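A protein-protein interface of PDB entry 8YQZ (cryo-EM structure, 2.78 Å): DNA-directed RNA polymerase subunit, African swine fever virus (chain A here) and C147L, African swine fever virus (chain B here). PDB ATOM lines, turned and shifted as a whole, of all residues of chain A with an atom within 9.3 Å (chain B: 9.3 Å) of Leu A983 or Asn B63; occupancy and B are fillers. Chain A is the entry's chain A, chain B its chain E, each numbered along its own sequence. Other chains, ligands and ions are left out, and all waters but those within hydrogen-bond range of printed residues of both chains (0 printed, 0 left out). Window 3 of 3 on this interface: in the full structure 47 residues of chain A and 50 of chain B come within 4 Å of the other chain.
Hydrophobic or aromatic side chains of chain B within 4 Å of the printed part of chain A: Ile B66 and Trp B136.
Hydrophobic or aromatic side chains of chain A within 4 Å of the printed part of chain B: Ile A976, Ile A979 and Leu A983.
Among the printed residues, 13 pairs touch across the chains.
Asn A978 touches none of the printed residues of chain B.
Of the printed residues of chain B, Gln A980 touches Asn B63 (3.3 Å), Glu B64 (3.7 Å), Arg B65 (2.8 Å) and Ile B66 (3.9 Å).
Glu A981 touches none of the printed residues of chain B.
Of the printed residues of chain B, Arg A982 touches Asn B63.
Of chain B, only Asn B63 (3.8 Å) comes within 4 Å of Leu A983.
Asn B63 touches just these residues of chain A: Gln A980, Arg A982 and Leu A983.
Printed residues of chain A within 4 Å of Arg B65: Asn A977 (3.0 Å), Ile A979 (3.6 Å) and Gln A980 (2.8 Å).
The nearest residue of chain B that does not touch Leu A983 is Glu B64 (6.0 Å).
The nearest printed residue of chain A that does not touch Trp B136 is Asn A978 (5.7 Å).
Among the printed residues, merely in contact across the chains: Ile A979 with Trp B136, Asn A977 with Ile B66, Ile A979 with Arg B65, Arg A982 with Asn B63, Gln A980 with Glu B64, Leu A983 with Asn B63, Ile A979 with Asp B62, Gln A980 with Ile B66 and Asn A977 with Trp B136.
The side-chain amide nitrogen (ND2) of Asn A977 is in hydrogen-bond range of the backbone carbonyl oxygen (O) of Arg B65, 3.0 Å away.
O of Asn B63 sits at hydrogen-bond distance from NE2 of Gln A980 (3.3 Å).
The side-chain amide nitrogen of Gln A980 is in hydrogen-bond range of the backbone carbonyl oxygen of Arg B65, at 2.8 Å.
The backbone carbonyl oxygen (O) of Ile A976 sits close to the backbone carbonyl oxygen (O) of Ile B66.
The side-chain carboxylate (OD2) of Asp B62 lies within salt-bridge range of the guanidinium group (NH1) of Arg B65 (3.9 Å).
The side-chain amide oxygen (OD1) of Asn A977 is in hydrogen-bond range of the backbone NH (N) of Ile A979.
OE1 of Glu B134 lies within hydrogen-bond range of NE1 of Trp B136, at 3.3 Å.
OD1 of Asn A977 sits at hydrogen-bond distance from N of Gln A980, 2.9 Å away.
The backbone carbonyl oxygen (O) of Ile B135 lies within hydrogen-bond range of the guanidinium group (NH1) of Arg B65 (2.6 Å).
OE1 of Gln A980 is in hydrogen-bond range of OG1 of Thr A985.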
ATOM      1  N   LYS A 969     -10.754 -22.471 -31.886  1.00  0.00           N
ATOM      2  CA  LYS A 969     -10.203 -22.078 -30.597  1.00  0.00           C
ATOM      3  C   LYS A 969     -10.488 -20.616 -30.300  1.00  0.00           C
ATOM      4  O   LYS A 969     -10.639 -20.234 -29.138  1.00  0.00           O
ATOM      5  CB  LYS A 969      -8.702 -22.355 -30.575  1.00  0.00           C
ATOM      6  CG  LYS A 969      -8.046 -22.168 -29.231  1.00  0.00           C
ATOM      7  CD  LYS A 969      -7.203 -20.909 -29.196  1.00  0.00           C
ATOM      8  CE  LYS A 969      -6.028 -21.001 -30.147  1.00  0.00           C
ATOM      9  NZ  LYS A 969      -5.212 -19.760 -30.140  1.00  0.00           N
ATOM     10  N   ASN A 970     -10.559 -19.782 -31.333  1.00  0.00           N
ATOM     11  CA  ASN A 970     -10.791 -18.353 -31.181  1.00  0.00           C
ATOM     12  C   ASN A 970     -12.240 -17.952 -31.387  1.00  0.00           C
ATOM     13  O   ASN A 970     -12.540 -16.759 -31.375  1.00  0.00           O
ATOM     14  CB  ASN A 970      -9.925 -17.568 -32.160  1.00  0.00           C
ATOM     15  CG  ASN A 970      -8.473 -17.602 -31.805  1.00  0.00           C
ATOM     16  OD1 ASN A 970      -8.102 -17.450 -30.650  1.00  0.00           O
ATOM     17  ND2 ASN A 970      -7.636 -17.813 -32.796  1.00  0.00           N
ATOM     18  N   TYR A 973     -14.398 -15.282 -29.202  1.00  0.00           N
ATOM     19  CA  TYR A 973     -14.095 -13.862 -29.293  1.00  0.00           C
ATOM     20  C   TYR A 973     -15.079 -13.112 -30.172  1.00  0.00           C
ATOM     21  O   TYR A 973     -15.028 -11.883 -30.217  1.00  0.00           O
ATOM     22  CB  TYR A 973     -12.686 -13.654 -29.828  1.00  0.00           C
ATOM     23  CG  TYR A 973     -11.594 -13.966 -28.842  1.00  0.00           C
ATOM     24  CD1 TYR A 973     -11.476 -13.263 -27.666  1.00  0.00           C
ATOM     25  CD2 TYR A 973     -10.665 -14.952 -29.105  1.00  0.00           C
ATOM     26  CE1 TYR A 973     -10.481 -13.544 -26.774  1.00  0.00           C
ATOM     27  CE2 TYR A 973      -9.664 -15.241 -28.220  1.00  0.00           C
ATOM     28  CZ  TYR A 973      -9.575 -14.532 -27.057  1.00  0.00           C
ATOM     29  OH  TYR A 973      -8.579 -14.812 -26.161  1.00  0.00           O
ATOM     30  N   ILE A 976     -16.668 -10.871 -27.893  1.00  0.00           N
ATOM     31  CA  ILE A 976     -15.979  -9.775 -27.228  1.00  0.00           C
ATOM     32  C   ILE A 976     -15.595  -8.684 -28.219  1.00  0.00           C
ATOM     33  O   ILE A 976     -16.356  -7.735 -28.409  1.00  0.00           O
ATOM     34  CB  ILE A 976     -14.742 -10.320 -26.487  1.00  0.00           C
ATOM     35  CG1 ILE A 976     -15.151 -11.501 -25.608  1.00  0.00           C
ATOM     36  CG2 ILE A 976     -14.077  -9.238 -25.670  1.00  0.00           C
ATOM     37  CD1 ILE A 976     -14.060 -12.440 -25.264  1.00  0.00           C
ATOM     38  N   ASN A 977     -14.490  -8.868 -28.942  1.00  0.00           N
ATOM     39  CA  ASN A 977     -14.055  -7.987 -30.025  1.00  0.00           C
ATOM     40  C   ASN A 977     -12.713  -8.449 -30.564  1.00  0.00           C
ATOM     41  O   ASN A 977     -12.128  -9.399 -30.043  1.00  0.00           O
ATOM     42  CB  ASN A 977     -13.991  -6.503 -29.625  1.00  0.00           C
ATOM     43  CG  ASN A 977     -13.091  -6.220 -28.452  1.00  0.00           C
ATOM     44  OD1 ASN A 977     -12.017  -6.776 -28.320  1.00  0.00           O
ATOM     45  ND2 ASN A 977     -13.507  -5.294 -27.623  1.00  0.00           N
ATOM     46  N   ASN A 978     -12.217  -7.786 -31.607  1.00  0.00           N
ATOM     47  CA  ASN A 978     -10.951  -8.156 -32.226  1.00  0.00           C
ATOM     48  C   ASN A 978      -9.735  -7.622 -31.481  1.00  0.00           C
ATOM     49  O   ASN A 978      -8.622  -8.069 -31.758  1.00  0.00           O
ATOM     50  CB  ASN A 978     -10.918  -7.682 -33.683  1.00  0.00           C
ATOM     51  CG  ASN A 978     -10.842  -6.169 -33.824  1.00  0.00           C
ATOM     52  OD1 ASN A 978     -11.051  -5.425 -32.874  1.00  0.00           O
ATOM     53  ND2 ASN A 978     -10.553  -5.713 -35.027  1.00  0.00           N
ATOM     54  N   ILE A 979      -9.914  -6.678 -30.557  1.00  0.00           N
ATOM     55  CA  ILE A 979      -8.795  -6.209 -29.747  1.00  0.00           C
ATOM     56  C   ILE A 979      -8.355  -7.291 -28.774  1.00  0.00           C
ATOM     57  O   ILE A 979      -7.160  -7.547 -28.606  1.00  0.00           O
ATOM     58  CB  ILE A 979      -9.172  -4.919 -28.998  1.00  0.00           C
ATOM     59  CG1 ILE A 979      -9.697  -3.853 -29.951  1.00  0.00           C
ATOM     60  CG2 ILE A 979      -7.998  -4.402 -28.202  1.00  0.00           C
ATOM     61  CD1 ILE A 979     -10.460  -2.783 -29.241  1.00  0.00           C
ATOM     62  N   GLN A 980      -9.315  -7.934 -28.108  1.00  0.00           N
ATOM     63  CA  GLN A 980      -8.983  -8.971 -27.144  1.00  0.00           C
ATOM     64  C   GLN A 980      -8.565 -10.269 -27.809  1.00  0.00           C
ATOM     65  O   GLN A 980      -7.831 -11.048 -27.203  1.00  0.00           O
ATOM     66  CB  GLN A 980     -10.162  -9.232 -26.215  1.00  0.00           C
ATOM     67  CG  GLN A 980     -10.700  -8.008 -25.526  1.00  0.00           C
ATOM     68  CD  GLN A 980      -9.674  -7.298 -24.683  1.00  0.00           C
ATOM     69  OE1 GLN A 980      -8.913  -7.918 -23.962  1.00  0.00           O
ATOM     70  NE2 GLN A 980      -9.656  -5.983 -24.764  1.00  0.00           N
ATOM     71  N   GLU A 981      -9.030 -10.532 -29.025  1.00  0.00           N
ATOM     72  CA  GLU A 981      -8.598 -11.727 -29.733  1.00  0.00           C
ATOM     73  C   GLU A 981      -7.139 -11.630 -30.137  1.00  0.00           C
ATOM     74  O   GLU A 981      -6.416 -12.629 -30.118  1.00  0.00           O
ATOM     75  CB  GLU A 981      -9.471 -11.954 -30.956  1.00  0.00           C
ATOM     76  CG  GLU A 981      -9.059 -13.137 -31.769  1.00  0.00           C
ATOM     77  CD  GLU A 981     -10.019 -13.413 -32.880  1.00  0.00           C
ATOM     78  OE1 GLU A 981     -11.034 -12.700 -32.965  1.00  0.00           O
ATOM     79  OE2 GLU A 981      -9.771 -14.347 -33.661  1.00  0.00           O
ATOM     80  N   ARG A 982      -6.694 -10.433 -30.518  1.00  0.00           N
ATOM     81  CA  ARG A 982      -5.293 -10.225 -30.859  1.00  0.00           C
ATOM     82  C   ARG A 982      -4.397 -10.416 -29.647  1.00  0.00           C
ATOM     83  O   ARG A 982      -3.309 -10.988 -29.753  1.00  0.00           O
ATOM     84  CB  ARG A 982      -5.108  -8.830 -31.444  1.00  0.00           C
ATOM     85  CG  ARG A 982      -3.696  -8.534 -31.884  1.00  0.00           C
ATOM     86  CD  ARG A 982      -3.540  -7.103 -32.348  1.00  0.00           C
ATOM     87  NE  ARG A 982      -3.591  -6.161 -31.239  1.00  0.00           N
ATOM     88  CZ  ARG A 982      -4.499  -5.207 -31.107  1.00  0.00           C
ATOM     89  NH1 ARG A 982      -5.454  -5.032 -32.005  1.00  0.00           N
ATOM     90  NH2 ARG A 982      -4.448  -4.409 -30.048  1.00  0.00           N
ATOM     91  N   LEU A 983      -4.831  -9.939 -28.484  1.00  0.00           N
ATOM     92  CA  LEU A 983      -4.041 -10.051 -27.269  1.00  0.00           C
ATOM     93  C   LEU A 983      -4.184 -11.397 -26.583  1.00  0.00           C
ATOM     94  O   LEU A 983      -3.434 -11.667 -25.642  1.00  0.00           O
ATOM     95  CB  LEU A 983      -4.423  -8.944 -26.295  1.00  0.00           C
ATOM     96  CG  LEU A 983      -4.233  -7.544 -26.849  1.00  0.00           C
ATOM     97  CD1 LEU A 983      -4.645  -6.523 -25.819  1.00  0.00           C
ATOM     98  CD2 LEU A 983      -2.801  -7.347 -27.276  1.00  0.00           C
ATOM     99  N   GLN A 984      -5.122 -12.229 -27.029  1.00  0.00           N
ATOM    100  CA  GLN A 984      -5.344 -13.575 -26.500  1.00  0.00           C
ATOM    101  C   GLN A 984      -5.536 -13.563 -24.989  1.00  0.00           C
ATOM    102  O   GLN A 984      -4.928 -14.338 -24.252  1.00  0.00           O
ATOM    103  CB  GLN A 984      -4.219 -14.516 -26.905  1.00  0.00           C
ATOM    104  CG  GLN A 984      -4.093 -14.666 -28.396  1.00  0.00           C
ATOM    105  CD  GLN A 984      -5.091 -15.649 -28.963  1.00  0.00           C
ATOM    106  OE1 GLN A 984      -5.053 -16.834 -28.656  1.00  0.00           O
ATOM    107  NE2 GLN A 984      -5.996 -15.156 -29.789  1.00  0.00           N
ATOM    108  N   THR A 985      -6.398 -12.664 -24.532  1.00  0.00           N
ATOM    109  CA  THR A 985      -6.760 -12.600 -23.134  1.00  0.00           C
ATOM    110  C   THR A 985      -7.712 -13.744 -22.785  1.00  0.00           C
ATOM    111  O   THR A 985      -8.322 -14.342 -23.672  1.00  0.00           O
ATOM    112  CB  THR A 985      -7.404 -11.253 -22.828  1.00  0.00           C
ATOM    113  OG1 THR A 985      -8.589 -11.112 -23.611  1.00  0.00           O
ATOM    114  CG2 THR A 985      -6.460 -10.127 -23.164  1.00  0.00           C
ATOM    115  N   PRO A 986      -7.836 -14.084 -21.503  1.00  0.00           N
ATOM    116  CA  PRO A 986      -8.708 -15.200 -21.119  1.00  0.00           C
ATOM    117  C   PRO A 986     -10.179 -14.952 -21.427  1.00  0.00           C
ATOM    118  O   PRO A 986     -10.662 -13.820 -21.416  1.00  0.00           O
ATOM    119  CB  PRO A 986      -8.463 -15.334 -19.613  1.00  0.00           C
ATOM    120  CG  PRO A 986      -7.809 -14.086 -19.206  1.00  0.00           C
ATOM    121  CD  PRO A 986      -7.018 -13.637 -20.367  1.00  0.00           C
ATOM    122  N   ILE A 987     -10.890 -16.040 -21.698  1.00  0.00           N
ATOM    123  CA  ILE A 987     -12.304 -16.008 -22.047  1.00  0.00           C
ATOM    124  C   ILE A 987     -13.123 -16.511 -20.866  1.00  0.00           C
ATOM    125  O   ILE A 987     -12.766 -17.525 -20.259  1.00  0.00           O
ATOM    126  CB  ILE A 987     -12.576 -16.845 -23.306  1.00  0.00           C
ATOM    127  CG1 ILE A 987     -11.630 -16.428 -24.425  1.00  0.00           C
ATOM    128  CG2 ILE A 987     -14.011 -16.692 -23.760  1.00  0.00           C
ATOM    129  CD1 ILE A 987     -11.707 -17.302 -25.640  1.00  0.00           C
ATOM    130  N   ILE B  59     -12.287   6.787 -18.345  1.00  0.00           N
ATOM    131  CA  ILE B  59     -12.308   6.247 -19.694  1.00  0.00           C
ATOM    132  C   ILE B  59     -11.431   5.009 -19.717  1.00  0.00           C
ATOM    133  O   ILE B  59     -10.230   5.087 -19.442  1.00  0.00           O
ATOM    134  CB  ILE B  59     -11.842   7.286 -20.722  1.00  0.00           C
ATOM    135  CG1 ILE B  59     -12.799   8.468 -20.721  1.00  0.00           C
ATOM    136  CG2 ILE B  59     -11.776   6.691 -22.095  1.00  0.00           C
ATOM    137  CD1 ILE B  59     -12.355   9.614 -21.554  1.00  0.00           C
ATOM    138  N   ILE B  60     -12.033   3.870 -20.040  1.00  0.00           N
ATOM    139  CA  ILE B  60     -11.284   2.614 -20.111  1.00  0.00           C
ATOM    140  C   ILE B  60     -10.243   2.715 -21.217  1.00  0.00           C
ATOM    141  O   ILE B  60     -10.571   3.154 -22.333  1.00  0.00           O
ATOM    142  CB  ILE B  60     -12.244   1.438 -20.353  1.00  0.00           C
ATOM    143  CG1 ILE B  60     -13.186   1.290 -19.167  1.00  0.00           C
ATOM    144  CG2 ILE B  60     -11.490   0.162 -20.584  1.00  0.00           C
ATOM    145  CD1 ILE B  60     -14.270   0.295 -19.382  1.00  0.00           C
ATOM    146  N   PRO B  61      -8.987   2.344 -20.971  1.00  0.00           N
ATOM    147  CA  PRO B  61      -7.965   2.452 -22.016  1.00  0.00           C
ATOM    148  C   PRO B  61      -8.249   1.540 -23.198  1.00  0.00           C
ATOM    149  O   PRO B  61      -8.873   0.490 -23.074  1.00  0.00           O
ATOM    150  CB  PRO B  61      -6.671   2.053 -21.294  1.00  0.00           C
ATOM    151  CG  PRO B  61      -7.096   1.424 -20.041  1.00  0.00           C
ATOM    152  CD  PRO B  61      -8.398   2.017 -19.667  1.00  0.00           C
ATOM    153  N   ASP B  62      -7.749   1.959 -24.361  1.00  0.00           N
ATOM    154  CA  ASP B  62      -8.156   1.362 -25.629  1.00  0.00           C
ATOM    155  C   ASP B  62      -7.889  -0.130 -25.696  1.00  0.00           C
ATOM    156  O   ASP B  62      -8.624  -0.854 -26.371  1.00  0.00           O
ATOM    157  CB  ASP B  62      -7.450   2.061 -26.786  1.00  0.00           C
ATOM    158  CG  ASP B  62      -8.169   3.308 -27.233  1.00  0.00           C
ATOM    159  OD1 ASP B  62      -7.699   3.947 -28.193  1.00  0.00           O
ATOM    160  OD2 ASP B  62      -9.210   3.643 -26.636  1.00  0.00           O
ATOM    161  N   ASN B  63      -6.852  -0.613 -25.022  1.00  0.00           N
ATOM    162  CA  ASN B  63      -6.521  -2.026 -25.106  1.00  0.00           C
ATOM    163  C   ASN B  63      -7.248  -2.873 -24.077  1.00  0.00           C
ATOM    164  O   ASN B  63      -7.016  -4.081 -24.022  1.00  0.00           O
ATOM    165  CB  ASN B  63      -5.017  -2.221 -24.970  1.00  0.00           C
ATOM    166  CG  ASN B  63      -4.326  -2.320 -26.310  1.00  0.00           C
ATOM    167  OD1 ASN B  63      -4.863  -1.903 -27.332  1.00  0.00           O
ATOM    168  ND2 ASN B  63      -3.127  -2.882 -26.313  1.00  0.00           N
ATOM    169  N   GLU B  64      -8.119  -2.279 -23.267  1.00  0.00           N
ATOM    170  CA  GLU B  64      -8.881  -3.011 -22.266  1.00  0.00           C
ATOM    171  C   GLU B  64     -10.371  -3.034 -22.565  1.00  0.00           C
ATOM    172  O   GLU B  64     -11.155  -3.470 -21.723  1.00  0.00           O
ATOM    173  CB  GLU B  64      -8.645  -2.414 -20.883  1.00  0.00           C
ATOM    174  CG  GLU B  64      -7.303  -2.721 -20.298  1.00  0.00           C
ATOM    175  CD  GLU B  64      -7.009  -1.864 -19.100  1.00  0.00           C
ATOM    176  OE1 GLU B  64      -7.965  -1.508 -18.386  1.00  0.00           O
ATOM    177  OE2 GLU B  64      -5.828  -1.543 -18.869  1.00  0.00           O
ATOM    178  N   ARG B  65     -10.779  -2.576 -23.742  1.00  0.00           N
ATOM    179  CA  ARG B  65     -12.190  -2.488 -24.077  1.00  0.00           C
ATOM    180  C   ARG B  65     -12.774  -3.863 -24.359  1.00  0.00           C
ATOM    181  O   ARG B  65     -12.160  -4.692 -25.032  1.00  0.00           O
ATOM    182  CB  ARG B  65     -12.393  -1.564 -25.274  1.00  0.00           C
ATOM    183  CG  ARG B  65     -12.192  -0.097 -24.946  1.00  0.00           C
ATOM    184  CD  ARG B  65     -12.443   0.780 -26.140  1.00  0.00           C
ATOM    185  NE  ARG B  65     -11.463   0.527 -27.181  1.00  0.00           N
ATOM    186  CZ  ARG B  65     -11.394   1.194 -28.320  1.00  0.00           C
ATOM    187  NH1 ARG B  65     -12.207   2.196 -28.580  1.00  0.00           N
ATOM    188  NH2 ARG B  65     -10.483   0.844 -29.220  1.00  0.00           N
ATOM    189  N   ILE B  66     -13.982  -4.087 -23.850  1.00  0.00           N
ATOM    190  CA  ILE B  66     -14.609  -5.395 -23.861  1.00  0.00           C
ATOM    191  C   ILE B  66     -15.760  -5.489 -24.859  1.00  0.00           C
ATOM    192  O   ILE B  66     -16.055  -6.584 -25.345  1.00  0.00           O
ATOM    193  CB  ILE B  66     -15.073  -5.746 -22.425  1.00  0.00           C
ATOM    194  CG1 ILE B  66     -13.909  -6.297 -21.608  1.00  0.00           C
ATOM    195  CG2 ILE B  66     -16.209  -6.715 -22.392  1.00  0.00           C
ATOM    196  CD1 ILE B  66     -12.931  -7.109 -22.402  1.00  0.00           C
ATOM    197  N   GLU B 134     -16.522   3.466 -22.207  1.00  0.00           N
ATOM    198  CA  GLU B 134     -15.705   3.074 -23.346  1.00  0.00           C
ATOM    199  C   GLU B 134     -16.030   4.001 -24.506  1.00  0.00           C
ATOM    200  O   GLU B 134     -17.201   4.174 -24.847  1.00  0.00           O
ATOM    201  CB  GLU B 134     -15.984   1.634 -23.754  1.00  0.00           C
ATOM    202  CG  GLU B 134     -15.206   0.601 -23.001  1.00  0.00           C
ATOM    203  CD  GLU B 134     -15.668  -0.796 -23.326  1.00  0.00           C
ATOM    204  OE1 GLU B 134     -16.453  -0.940 -24.275  1.00  0.00           O
ATOM    205  OE2 GLU B 134     -15.255  -1.750 -22.642  1.00  0.00           O
ATOM    206  N   ILE B 135     -15.006   4.598 -25.105  1.00  0.00           N
ATOM    207  CA  ILE B 135     -15.173   5.479 -26.255  1.00  0.00           C
ATOM    208  C   ILE B 135     -14.807   4.694 -27.501  1.00  0.00           C
ATOM    209  O   ILE B 135     -13.721   4.114 -27.579  1.00  0.00           O
ATOM    210  CB  ILE B 135     -14.303   6.740 -26.145  1.00  0.00           C
ATOM    211  CG1 ILE B 135     -14.518   7.468 -24.823  1.00  0.00           C
ATOM    212  CG2 ILE B 135     -14.602   7.677 -27.296  1.00  0.00           C
ATOM    213  CD1 ILE B 135     -15.768   8.216 -24.744  1.00  0.00           C
ATOM    214  N   TRP B 136     -15.692   4.689 -28.485  1.00  0.00           N
ATOM    215  CA  TRP B 136     -15.483   3.954 -29.721  1.00  0.00           C
ATOM    216  C   TRP B 136     -15.541   4.919 -30.891  1.00  0.00           C
ATOM    217  O   TRP B 136     -16.381   5.819 -30.916  1.00  0.00           O
ATOM    218  CB  TRP B 136     -16.523   2.839 -29.870  1.00  0.00           C
ATOM    219  CG  TRP B 136     -16.187   1.629 -29.068  1.00  0.00           C
ATOM    220  CD1 TRP B 136     -16.627   1.334 -27.824  1.00  0.00           C
ATOM    221  CD2 TRP B 136     -15.336   0.550 -29.459  1.00  0.00           C
ATOM    222  NE1 TRP B 136     -16.103   0.145 -27.408  1.00  0.00           N
ATOM    223  CE2 TRP B 136     -15.309  -0.361 -28.399  1.00  0.00           C
ATOM    224  CE3 TRP B 136     -14.595   0.269 -30.606  1.00  0.00           C
ATOM    225  CZ2 TRP B 136     -14.572  -1.529 -28.445  1.00  0.00           C
ATOM    226  CZ3 TRP B 136     -13.870  -0.893 -30.650  1.00  0.00           C
ATOM    227  CH2 TRP B 136     -13.859  -1.774 -29.578  1.00  0.00           C
